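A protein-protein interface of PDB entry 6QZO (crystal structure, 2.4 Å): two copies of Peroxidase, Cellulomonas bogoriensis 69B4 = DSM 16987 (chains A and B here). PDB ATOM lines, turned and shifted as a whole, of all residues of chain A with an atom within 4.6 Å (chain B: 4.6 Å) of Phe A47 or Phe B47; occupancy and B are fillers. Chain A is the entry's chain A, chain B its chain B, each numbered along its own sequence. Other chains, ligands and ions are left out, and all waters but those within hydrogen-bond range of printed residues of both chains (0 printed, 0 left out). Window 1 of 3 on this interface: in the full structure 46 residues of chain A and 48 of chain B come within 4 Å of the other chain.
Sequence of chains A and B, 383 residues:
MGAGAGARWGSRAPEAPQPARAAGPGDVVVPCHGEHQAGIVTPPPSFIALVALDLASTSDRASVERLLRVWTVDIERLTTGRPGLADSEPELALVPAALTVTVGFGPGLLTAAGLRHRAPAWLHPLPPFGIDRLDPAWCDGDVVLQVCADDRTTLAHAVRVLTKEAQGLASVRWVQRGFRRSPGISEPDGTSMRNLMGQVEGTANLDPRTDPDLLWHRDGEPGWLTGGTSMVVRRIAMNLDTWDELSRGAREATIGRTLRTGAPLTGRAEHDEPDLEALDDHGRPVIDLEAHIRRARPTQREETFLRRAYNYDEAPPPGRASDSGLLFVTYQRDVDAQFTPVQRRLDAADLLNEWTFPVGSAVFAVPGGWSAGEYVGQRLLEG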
ATOM      1  N   PRO A  45     -33.498 -21.282   8.006  1.00  0.00           N
ATOM      2  CA  PRO A  45     -33.395 -22.627   8.565  1.00  0.00           C
ATOM      3  C   PRO A  45     -32.090 -22.783   9.361  1.00  0.00           C
ATOM      4  O   PRO A  45     -31.327 -21.844   9.432  1.00  0.00           O
ATOM      5  CB  PRO A  45     -33.393 -23.474   7.287  1.00  0.00           C
ATOM      6  CG  PRO A  45     -32.580 -22.640   6.333  1.00  0.00           C
ATOM      7  CD  PRO A  45     -33.014 -21.225   6.609  1.00  0.00           C
ATOM      8  N   SER A  46     -31.843 -23.979   9.891  1.00  0.00           N
ATOM      9  CA  SER A  46     -30.809 -24.243  10.924  1.00  0.00           C
ATOM     10  C   SER A  46     -29.390 -24.000  10.396  1.00  0.00           C
ATOM     11  O   SER A  46     -28.552 -23.521  11.197  1.00  0.00           O
ATOM     12  CB  SER A  46     -30.967 -25.627  11.475  1.00  0.00           C
ATOM     13  OG  SER A  46     -32.195 -25.756  12.168  1.00  0.00           O
ATOM     14  N   PHE A  47     -29.090 -24.321   9.133  1.00  0.00           N
ATOM     15  CA  PHE A  47     -27.682 -24.343   8.648  1.00  0.00           C
ATOM     16  C   PHE A  47     -27.495 -23.521   7.373  1.00  0.00           C
ATOM     17  O   PHE A  47     -28.462 -23.361   6.590  1.00  0.00           O
ATOM     18  CB  PHE A  47     -27.215 -25.784   8.463  1.00  0.00           C
ATOM     19  CG  PHE A  47     -27.505 -26.619   9.679  1.00  0.00           C
ATOM     20  CD1 PHE A  47     -26.904 -26.316  10.893  1.00  0.00           C
ATOM     21  CD2 PHE A  47     -28.440 -27.634   9.638  1.00  0.00           C
ATOM     22  CE1 PHE A  47     -27.202 -27.046  12.035  1.00  0.00           C
ATOM     23  CE2 PHE A  47     -28.726 -28.373  10.779  1.00  0.00           C
ATOM     24  CZ  PHE A  47     -28.113 -28.073  11.978  1.00  0.00           C
ATOM     25  N   ILE A  48     -26.256 -23.044   7.199  1.00  0.00           N
ATOM     26  CA  ILE A  48     -25.780 -22.222   6.052  1.00  0.00           C
ATOM     27  C   ILE A  48     -24.352 -22.623   5.675  1.00  0.00           C
ATOM     28  O   ILE A  48     -23.527 -22.851   6.576  1.00  0.00           O
ATOM     29  CB  ILE A  48     -25.822 -20.716   6.372  1.00  0.00           C
ATOM     30  CG1 ILE A  48     -25.595 -19.887   5.115  1.00  0.00           C
ATOM     31  CG2 ILE A  48     -24.837 -20.344   7.479  1.00  0.00           C
ATOM     32  CD1 ILE A  48     -26.083 -18.459   5.254  1.00  0.00           C
ATOM     33  N   VAL A 147     -26.026 -21.459   0.538  1.00  0.00           N
ATOM     34  CA  VAL A 147     -26.738 -22.766   0.620  1.00  0.00           C
ATOM     35  C   VAL A 147     -27.233 -22.930   2.056  1.00  0.00           C
ATOM     36  O   VAL A 147     -26.375 -22.951   3.003  1.00  0.00           O
ATOM     37  CB  VAL A 147     -25.835 -23.936   0.196  1.00  0.00           C
ATOM     38  CG1 VAL A 147     -26.627 -25.221  -0.009  1.00  0.00           C
ATOM     39  CG2 VAL A 147     -25.054 -23.595  -1.057  1.00  0.00           C
ATOM     40  N   CYS A 148     -28.560 -23.009   2.204  1.00  0.00           N
ATOM     41  CA  CYS A 148     -29.260 -23.071   3.509  1.00  0.00           C
ATOM     42  C   CYS A 148     -30.151 -24.308   3.555  1.00  0.00           C
ATOM     43  O   CYS A 148     -30.831 -24.554   2.543  1.00  0.00           O
ATOM     44  CB  CYS A 148     -30.139 -21.849   3.705  1.00  0.00           C
ATOM     45  SG  CYS A 148     -29.173 -20.354   3.982  1.00  0.00           S
ATOM     46  N   ALA A 149     -30.176 -25.001   4.695  1.00  0.00           N
ATOM     47  CA  ALA A 149     -31.038 -26.184   4.925  1.00  0.00           C
ATOM     48  C   ALA A 149     -31.169 -26.492   6.418  1.00  0.00           C
ATOM     49  O   ALA A 149     -30.334 -26.035   7.218  1.00  0.00           O
ATOM     50  CB  ALA A 149     -30.507 -27.374   4.169  1.00  0.00           C
ATOM     51  N   ASP A 150     -32.195 -27.262   6.764  1.00  0.00           N
ATOM     52  CA  ASP A 150     -32.477 -27.723   8.146  1.00  0.00           C
ATOM     53  C   ASP A 150     -31.761 -29.048   8.417  1.00  0.00           C
ATOM     54  O   ASP A 150     -32.063 -29.653   9.460  1.00  0.00           O
ATOM     55  CB  ASP A 150     -33.985 -27.868   8.373  1.00  0.00           C
ATOM     56  CG  ASP A 150     -34.655 -26.591   8.813  1.00  0.00           C
ATOM     57  OD1 ASP A 150     -33.957 -25.754   9.442  1.00  0.00           O
ATOM     58  OD2 ASP A 150     -35.861 -26.443   8.529  1.00  0.00           O
ATOM     59  N   ASP A 151     -30.868 -29.481   7.524  1.00  0.00           N
ATOM     60  CA  ASP A 151     -30.115 -30.757   7.661  1.00  0.00           C
ATOM     61  C   ASP A 151     -28.724 -30.624   7.042  1.00  0.00           C
ATOM     62  O   ASP A 151     -28.626 -30.164   5.912  1.00  0.00           O
ATOM     63  CB  ASP A 151     -30.866 -31.919   7.015  1.00  0.00           C
ATOM     64  CG  ASP A 151     -30.213 -33.254   7.332  1.00  0.00           C
ATOM     65  OD1 ASP A 151     -29.270 -33.633   6.609  1.00  0.00           O
ATOM     66  OD2 ASP A 151     -30.608 -33.870   8.356  1.00  0.00           O
ATOM     67  N   ARG A 152     -27.695 -31.082   7.759  1.00  0.00           N
ATOM     68  CA  ARG A 152     -26.264 -30.873   7.437  1.00  0.00           C
ATOM     69  C   ARG A 152     -25.814 -31.837   6.332  1.00  0.00           C
ATOM     70  O   ARG A 152     -24.900 -31.473   5.567  1.00  0.00           O
ATOM     71  CB  ARG A 152     -25.425 -31.006   8.698  1.00  0.00           C
ATOM     72  CG  ARG A 152     -24.023 -30.471   8.536  1.00  0.00           C
ATOM     73  CD  ARG A 152     -23.883 -29.001   8.211  1.00  0.00           C
ATOM     74  NE  ARG A 152     -22.450 -28.858   8.086  1.00  0.00           N
ATOM     75  CZ  ARG A 152     -21.695 -29.171   7.017  1.00  0.00           C
ATOM     76  NH1 ARG A 152     -22.217 -29.671   5.905  1.00  0.00           N
ATOM     77  NH2 ARG A 152     -20.388 -29.017   7.102  1.00  0.00           N
ATOM     78  N   LEU A 155     -27.137 -30.390   3.138  1.00  0.00           N
ATOM     79  CA  LEU A 155     -26.313 -29.191   2.835  1.00  0.00           C
ATOM     80  C   LEU A 155     -24.973 -29.638   2.242  1.00  0.00           C
ATOM     81  O   LEU A 155     -24.552 -29.072   1.200  1.00  0.00           O
ATOM     82  CB  LEU A 155     -26.136 -28.399   4.131  1.00  0.00           C
ATOM     83  CG  LEU A 155     -25.472 -27.036   3.981  1.00  0.00           C
ATOM     84  CD1 LEU A 155     -26.326 -26.165   3.135  1.00  0.00           C
ATOM     85  CD2 LEU A 155     -25.256 -26.375   5.337  1.00  0.00           C
ATOM     86  N   GLY A 178     -22.202 -21.950   9.065  1.00  0.00           N
ATOM     87  CA  GLY A 178     -22.826 -21.399  10.277  1.00  0.00           C
ATOM     88  C   GLY A 178     -24.067 -22.179  10.651  1.00  0.00           C
ATOM     89  O   GLY A 178     -24.491 -23.054   9.843  1.00  0.00           O
ATOM     90  N   PHE A 179     -24.641 -21.839  11.811  1.00  0.00           N
ATOM     91  CA  PHE A 179     -25.749 -22.587  12.435  1.00  0.00           C
ATOM     92  C   PHE A 179     -26.577 -21.680  13.346  1.00  0.00           C
ATOM     93  O   PHE A 179     -26.086 -20.639  13.855  1.00  0.00           O
ATOM     94  CB  PHE A 179     -25.208 -23.768  13.243  1.00  0.00           C
ATOM     95  CG  PHE A 179     -24.221 -23.412  14.324  1.00  0.00           C
ATOM     96  CD1 PHE A 179     -24.654 -23.065  15.595  1.00  0.00           C
ATOM     97  CD2 PHE A 179     -22.858 -23.451  14.079  1.00  0.00           C
ATOM     98  CE1 PHE A 179     -23.751 -22.755  16.595  1.00  0.00           C
ATOM     99  CE2 PHE A 179     -21.956 -23.147  15.086  1.00  0.00           C
ATOM    100  CZ  PHE A 179     -22.401 -22.797  16.341  1.00  0.00           C
ATOM    101  N   ARG A 180     -27.839 -22.076  13.496  1.00  0.00           N
ATOM    102  CA  ARG A 180     -28.759 -21.656  14.577  1.00  0.00           C
ATOM    103  C   ARG A 180     -29.188 -22.945  15.276  1.00  0.00           C
ATOM    104  O   ARG A 180     -28.548 -23.988  15.032  1.00  0.00           O
ATOM    105  CB  ARG A 180     -29.970 -20.915  14.004  1.00  0.00           C
ATOM    106  CG  ARG A 180     -29.614 -19.754  13.081  1.00  0.00           C
ATOM    107  CD  ARG A 180     -30.866 -19.138  12.472  1.00  0.00           C
ATOM    108  NE  ARG A 180     -30.530 -17.896  11.789  1.00  0.00           N
ATOM    109  CZ  ARG A 180     -31.278 -16.796  11.759  1.00  0.00           C
ATOM    110  NH1 ARG A 180     -32.439 -16.727  12.399  1.00  0.00           N
ATOM    111  NH2 ARG A 180     -30.838 -15.738  11.100  1.00  0.00           N
ATOM    112  N   SER A 182     -31.489 -26.341  15.948  1.00  0.00           N
ATOM    113  CA  SER A 182     -31.950 -27.413  15.039  1.00  0.00           C
ATOM    114  C   SER A 182     -33.449 -27.274  14.791  1.00  0.00           C
ATOM    115  O   SER A 182     -34.156 -26.602  15.539  1.00  0.00           O
ATOM    116  CB  SER A 182     -31.576 -28.747  15.611  1.00  0.00           C
ATOM    117  OG  SER A 182     -30.154 -28.899  15.570  1.00  0.00           O
ATOM    118  N   TYR A 310     -25.876 -15.934  11.033  1.00  0.00           N
ATOM    119  CA  TYR A 310     -25.667 -17.312  11.529  1.00  0.00           C
ATOM    120  C   TYR A 310     -24.459 -17.302  12.469  1.00  0.00           C
ATOM    121  O   TYR A 310     -23.587 -16.443  12.305  1.00  0.00           O
ATOM    122  CB  TYR A 310     -25.472 -18.255  10.337  1.00  0.00           C
ATOM    123  CG  TYR A 310     -26.754 -18.692   9.679  1.00  0.00           C
ATOM    124  CD1 TYR A 310     -27.422 -17.884   8.767  1.00  0.00           C
ATOM    125  CD2 TYR A 310     -27.316 -19.910   9.991  1.00  0.00           C
ATOM    126  CE1 TYR A 310     -28.617 -18.285   8.192  1.00  0.00           C
ATOM    127  CE2 TYR A 310     -28.503 -20.328   9.417  1.00  0.00           C
ATOM    128  CZ  TYR A 310     -29.149 -19.523   8.510  1.00  0.00           C
ATOM    129  OH  TYR A 310     -30.312 -19.970   7.965  1.00  0.00           O
ATOM    130  N   PRO B  45     -27.017 -38.931  18.811  1.00  0.00           N
ATOM    131  CA  PRO B  45     -27.735 -37.739  18.380  1.00  0.00           C
ATOM    132  C   PRO B  45     -27.043 -37.102  17.169  1.00  0.00           C
ATOM    133  O   PRO B  45     -26.024 -37.609  16.734  1.00  0.00           O
ATOM    134  CB  PRO B  45     -27.633 -36.860  19.629  1.00  0.00           C
ATOM    135  CG  PRO B  45     -26.248 -37.151  20.131  1.00  0.00           C
ATOM    136  CD  PRO B  45     -26.080 -38.648  19.916  1.00  0.00           C
ATOM    137  N   SER B  46     -27.574 -35.974  16.688  1.00  0.00           N
ATOM    138  CA  SER B  46     -27.222 -35.382  15.370  1.00  0.00           C
ATOM    139  C   SER B  46     -25.759 -34.911  15.320  1.00  0.00           C
ATOM    140  O   SER B  46     -25.159 -35.042  14.218  1.00  0.00           O
ATOM    141  CB  SER B  46     -28.165 -34.273  15.033  1.00  0.00           C
ATOM    142  OG  SER B  46     -29.480 -34.795  14.851  1.00  0.00           O
ATOM    143  N   PHE B  47     -25.193 -34.376  16.408  1.00  0.00           N
ATOM    144  CA  PHE B  47     -23.873 -33.684  16.333  1.00  0.00           C
ATOM    145  C   PHE B  47     -22.885 -34.205  17.374  1.00  0.00           C
ATOM    146  O   PHE B  47     -23.311 -34.694  18.433  1.00  0.00           O
ATOM    147  CB  PHE B  47     -24.064 -32.168  16.453  1.00  0.00           C
ATOM    148  CG  PHE B  47     -25.119 -31.671  15.505  1.00  0.00           C
ATOM    149  CD1 PHE B  47     -24.940 -31.792  14.140  1.00  0.00           C
ATOM    150  CD2 PHE B  47     -26.322 -31.182  15.970  1.00  0.00           C
ATOM    151  CE1 PHE B  47     -25.926 -31.380  13.252  1.00  0.00           C
ATOM    152  CE2 PHE B  47     -27.306 -30.760  15.087  1.00  0.00           C
ATOM    153  CZ  PHE B  47     -27.110 -30.869  13.729  1.00  0.00           C
ATOM    154  N   ILE B  48     -21.595 -34.062  17.042  1.00  0.00           N
ATOM    155  CA  ILE B  48     -20.416 -34.485  17.849  1.00  0.00           C
ATOM    156  C   ILE B  48     -19.292 -33.457  17.696  1.00  0.00           C
ATOM    157  O   ILE B  48     -19.049 -32.971  16.579  1.00  0.00           O
ATOM    158  CB  ILE B  48     -19.905 -35.880  17.423  1.00  0.00           C
ATOM    159  CG1 ILE B  48     -18.856 -36.402  18.410  1.00  0.00           C
ATOM    160  CG2 ILE B  48     -19.354 -35.874  16.010  1.00  0.00           C
ATOM    161  CD1 ILE B  48     -18.686 -37.907  18.338  1.00  0.00           C
ATOM    162  N   VAL B 147     -18.215 -34.824  22.947  1.00  0.00           N
ATOM    163  CA  VAL B 147     -19.400 -33.978  23.258  1.00  0.00           C
ATOM    164  C   VAL B 147     -20.409 -34.166  22.126  1.00  0.00           C
ATOM    165  O   VAL B 147     -20.066 -33.857  20.946  1.00  0.00           O
ATOM    166  CB  VAL B 147     -19.017 -32.498  23.436  1.00  0.00           C
ATOM    167  CG1 VAL B 147     -20.154 -31.673  24.031  1.00  0.00           C
ATOM    168  CG2 VAL B 147     -17.762 -32.362  24.264  1.00  0.00           C
ATOM    169  N   CYS B 148     -21.588 -34.677  22.470  1.00  0.00           N
ATOM    170  CA  CYS B 148     -22.675 -35.036  21.534  1.00  0.00           C
ATOM    171  C   CYS B 148     -23.966 -34.328  21.941  1.00  0.00           C
ATOM    172  O   CYS B 148     -24.248 -34.319  23.147  1.00  0.00           O
ATOM    173  CB  CYS B 148     -22.933 -36.535  21.561  1.00  0.00           C
ATOM    174  SG  CYS B 148     -21.579 -37.475  20.833  1.00  0.00           S
ATOM    175  N   ALA B 149     -24.721 -33.813  20.973  1.00  0.00           N
ATOM    176  CA  ALA B 149     -26.039 -33.179  21.186  1.00  0.00           C
ATOM    177  C   ALA B 149     -26.840 -33.101  19.874  1.00  0.00           C
ATOM    178  O   ALA B 149     -26.259 -33.215  18.782  1.00  0.00           O
ATOM    179  CB  ALA B 149     -25.864 -31.820  21.794  1.00  0.00           C
ATOM    180  N   ASP B 150     -28.146 -32.902  20.003  1.00  0.00           N
ATOM    181  CA  ASP B 150     -29.099 -32.746  18.873  1.00  0.00           C
ATOM    182  C   ASP B 150     -29.198 -31.278  18.459  1.00  0.00           C
ATOM    183  O   ASP B 150     -30.105 -30.980  17.648  1.00  0.00           O
ATOM    184  CB  ASP B 150     -30.471 -33.302  19.242  1.00  0.00           C
ATOM    185  CG  ASP B 150     -30.610 -34.784  18.974  1.00  0.00           C
ATOM    186  OD1 ASP B 150     -29.908 -35.269  18.049  1.00  0.00           O
ATOM    187  OD2 ASP B 150     -31.416 -35.434  19.686  1.00  0.00           O
ATOM    188  N   ASP B 151     -28.319 -30.414  18.985  1.00  0.00           N
ATOM    189  CA  ASP B 151     -28.334 -28.959  18.696  1.00  0.00           C
ATOM    190  C   ASP B 151     -26.908 -28.403  18.741  1.00  0.00           C
ATOM    191  O   ASP B 151     -26.207 -28.668  19.725  1.00  0.00           O
ATOM    192  CB  ASP B 151     -29.218 -28.195  19.675  1.00  0.00           C
ATOM    193  CG  ASP B 151     -29.402 -26.755  19.249  1.00  0.00           C
ATOM    194  OD1 ASP B 151     -28.521 -25.920  19.605  1.00  0.00           O
ATOM    195  OD2 ASP B 151     -30.391 -26.490  18.513  1.00  0.00           O
ATOM    196  N   ARG B 152     -26.541 -27.601  17.729  1.00  0.00           N
ATOM    197  CA  ARG B 152     -25.160 -27.126  17.483  1.00  0.00           C
ATOM    198  C   ARG B 152     -24.802 -25.980  18.437  1.00  0.00           C
ATOM    199  O   ARG B 152     -23.617 -25.838  18.768  1.00  0.00           O
ATOM    200  CB  ARG B 152     -25.045 -26.700  16.021  1.00  0.00           C
ATOM    201  CG  ARG B 152     -23.628 -26.469  15.562  1.00  0.00           C
ATOM    202  CD  ARG B 152     -22.747 -27.683  15.573  1.00  0.00           C
ATOM    203  NE  ARG B 152     -21.482 -27.139  15.099  1.00  0.00           N
ATOM    204  CZ  ARG B 152     -20.508 -26.612  15.868  1.00  0.00           C
ATOM    205  NH1 ARG B 152     -19.441 -26.086  15.277  1.00  0.00           N
ATOM    206  NH2 ARG B 152     -20.592 -26.585  17.200  1.00  0.00           N
ATOM    207  N   LEU B 155     -24.070 -27.561  21.763  1.00  0.00           N
ATOM    208  CA  LEU B 155     -22.760 -28.245  21.634  1.00  0.00           C
ATOM    209  C   LEU B 155     -21.648 -27.198  21.720  1.00  0.00           C
ATOM    210  O   LEU B 155     -20.655 -27.429  22.479  1.00  0.00           O
ATOM    211  CB  LEU B 155     -22.744 -28.991  20.297  1.00  0.00           C
ATOM    212  CG  LEU B 155     -21.524 -29.871  20.029  1.00  0.00           C
ATOM    213  CD1 LEU B 155     -21.433 -30.961  21.053  1.00  0.00           C
ATOM    214  CD2 LEU B 155     -21.571 -30.471  18.654  1.00  0.00           C
ATOM    215  N   GLY B 178     -18.495 -33.410  13.711  1.00  0.00           N
ATOM    216  CA  GLY B 178     -19.212 -34.297  12.781  1.00  0.00           C
ATOM    217  C   GLY B 178     -20.708 -34.193  12.964  1.00  0.00           C
ATOM    218  O   GLY B 178     -21.139 -33.541  13.936  1.00  0.00           O
ATOM    219  N   PHE B 179     -21.449 -34.858  12.080  1.00  0.00           N
ATOM    220  CA  PHE B 179     -22.919 -34.737  11.962  1.00  0.00           C
ATOM    221  C   PHE B 179     -23.524 -35.996  11.347  1.00  0.00           C
ATOM    222  O   PHE B 179     -22.842 -36.752  10.613  1.00  0.00           O
ATOM    223  CB  PHE B 179     -23.296 -33.522  11.117  1.00  0.00           C
ATOM    224  CG  PHE B 179     -22.720 -33.498   9.725  1.00  0.00           C
ATOM    225  CD1 PHE B 179     -23.373 -34.122   8.676  1.00  0.00           C
ATOM    226  CD2 PHE B 179     -21.540 -32.829   9.456  1.00  0.00           C
ATOM    227  CE1 PHE B 179     -22.858 -34.092   7.391  1.00  0.00           C
ATOM    228  CE2 PHE B 179     -21.027 -32.795   8.166  1.00  0.00           C
ATOM    229  CZ  PHE B 179     -21.688 -33.426   7.137  1.00  0.00           C
ATOM    230  N   ARG B 180     -24.787 -36.216  11.703  1.00  0.00           N
ATOM    231  CA  ARG B 180     -25.737 -37.106  10.991  1.00  0.00           C
ATOM    232  C   ARG B 180     -26.920 -36.215  10.604  1.00  0.00           C
ATOM    233  O   ARG B 180     -26.772 -34.973  10.682  1.00  0.00           O
ATOM    234  CB  ARG B 180     -26.198 -38.253  11.892  1.00  0.00           C
ATOM    235  CG  ARG B 180     -25.070 -39.012  12.572  1.00  0.00           C
ATOM    236  CD  ARG B 180     -25.596 -40.089  13.502  1.00  0.00           C
ATOM    237  NE  ARG B 180     -24.519 -40.987  13.892  1.00  0.00           N
ATOM    238  CZ  ARG B 180     -24.636 -42.296  14.096  1.00  0.00           C
ATOM    239  NH1 ARG B 180     -25.797 -42.920  13.946  1.00  0.00           N
ATOM    240  NH2 ARG B 180     -23.564 -42.986  14.444  1.00  0.00           N
ATOM    241  N   SER B 182     -30.562 -34.272  11.151  1.00  0.00           N
ATOM    242  CA  SER B 182     -31.085 -33.458  12.271  1.00  0.00           C
ATOM    243  C   SER B 182     -32.142 -34.256  13.034  1.00  0.00           C
ATOM    244  O   SER B 182     -32.690 -35.232  12.530  1.00  0.00           O
ATOM    245  CB  SER B 182     -31.616 -32.150  11.754  1.00  0.00           C
ATOM    246  OG  SER B 182     -30.543 -31.362  11.282  1.00  0.00           O
ATOM    247  N   TYR B 310     -19.537 -40.600  12.694  1.00  0.00           N
ATOM    248  CA  TYR B 310     -20.152 -39.310  12.305  1.00  0.00           C
ATOM    249  C   TYR B 310     -19.509 -38.862  10.987  1.00  0.00           C
ATOM    250  O   TYR B 310     -18.355 -39.238  10.730  1.00  0.00           O
ATOM    251  CB  TYR B 310     -19.975 -38.278  13.417  1.00  0.00           C
ATOM    252  CG  TYR B 310     -20.979 -38.403  14.534  1.00  0.00           C
ATOM    253  CD1 TYR B 310     -20.833 -39.338  15.545  1.00  0.00           C
ATOM    254  CD2 TYR B 310     -22.100 -37.601  14.566  1.00  0.00           C
ATOM    255  CE1 TYR B 310     -21.779 -39.470  16.551  1.00  0.00           C
ATOM    256  CE2 TYR B 310     -23.041 -37.703  15.573  1.00  0.00           C
ATOM    257  CZ  TYR B 310     -22.883 -38.644  16.563  1.00  0.00           C
ATOM    258  OH  TYR B 310     -23.816 -38.700  17.560  1.00  0.00           O
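Of the 16 printed residues of chain B, 6 touch a printed residue of chain A.
Printed residues of chain B that touch a printed residue of chain A: Phe B47, Asp B150, Asp B151, Arg B152, Phe B179 and Ser B182.
Hydrophobic or aromatic side chains of chain B that line the printed part of chain A: Phe B47 and Phe B179.
Of the 16 printed residues of chain A, 6 touch a printed residue of chain B.
Among the printed residues, no Asp or Glu carboxylate lies within 4 Å of a Lys or Arg side-chain nitrogen of the other chain.
Phe A47 touches Ser B182, and with the chains exchanged Ser A182 touches Phe B47.
Asp A150 touches Ser B182, and with the chains exchanged Ser A182 touches Asp B150.
Asp A151 touches Ser B182, and with the chains exchanged Ser A182 touches Asp B151.
Arg A152 touches Phe B179, and with the chains exchanged Phe A179 touches Arg B152.
Of chain B, only Phe B47 and Ser B182 come within 4 Å of Phe A47.
Of the printed residues of chain A, Asp B151 touches Ser A182 (2.8 Å).
Printed residues of chain B within 4 Å of Asp A151: Ser B182.
Of the printed residues of chain B, Asp A150 touches Ser B182 (2.9 Å).
Of the printed residues of chain A, Ser B182 touches Phe A47 (3.5 Å), Asp A150 (2.9 Å) and Asp A151 (2.8 Å).
The nearest printed residue of chain A that does not touch Arg B152 is Ser A182 (4.4 Å).
Phe A47 touches Phe B47 (CZ to CZ, 3.4 Å).
CE2 of Phe A47 touches OG of Ser B182, 3.5 Å away.
Arg A152 touches Phe B179 (CG to CG, 3.5 Å).
Phe A179 touches Arg B152 (CG to CG, 3.4 Å).
CE2 of Phe B47 touches OG of Ser A182 (3.4 Å).
O of Ala B149 is in hydrogen-bond range of N of Phe B47 (2.8 Å).
N of Ser B46 lies within hydrogen-bond range of OD1 of Asp B150, at 2.8 Å.
N of Phe A47 is in hydrogen-bond range of O of Ala A149 (2.9 Å).
N of Ser A46 lies within hydrogen-bond range of OD1 of Asp A150 (2.8 Å).
The side-chain hydroxyl (OG) of Ser A182 lies within hydrogen-bond range of the backbone carbonyl oxygen (O) of Asp B150, 2.9 Å away.
The side-chain carboxylate (OD2) of Asp A151 sits at hydrogen-bond distance from the backbone NH (N) of Ser B182, 2.8 Å away.
The backbone NH (N) of Ser A182 lies within hydrogen-bond range of the side-chain carboxylate (OD2) of Asp B151.
O of Asp A150 is in hydrogen-bond range of OG of Ser B182 (2.9 Å).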
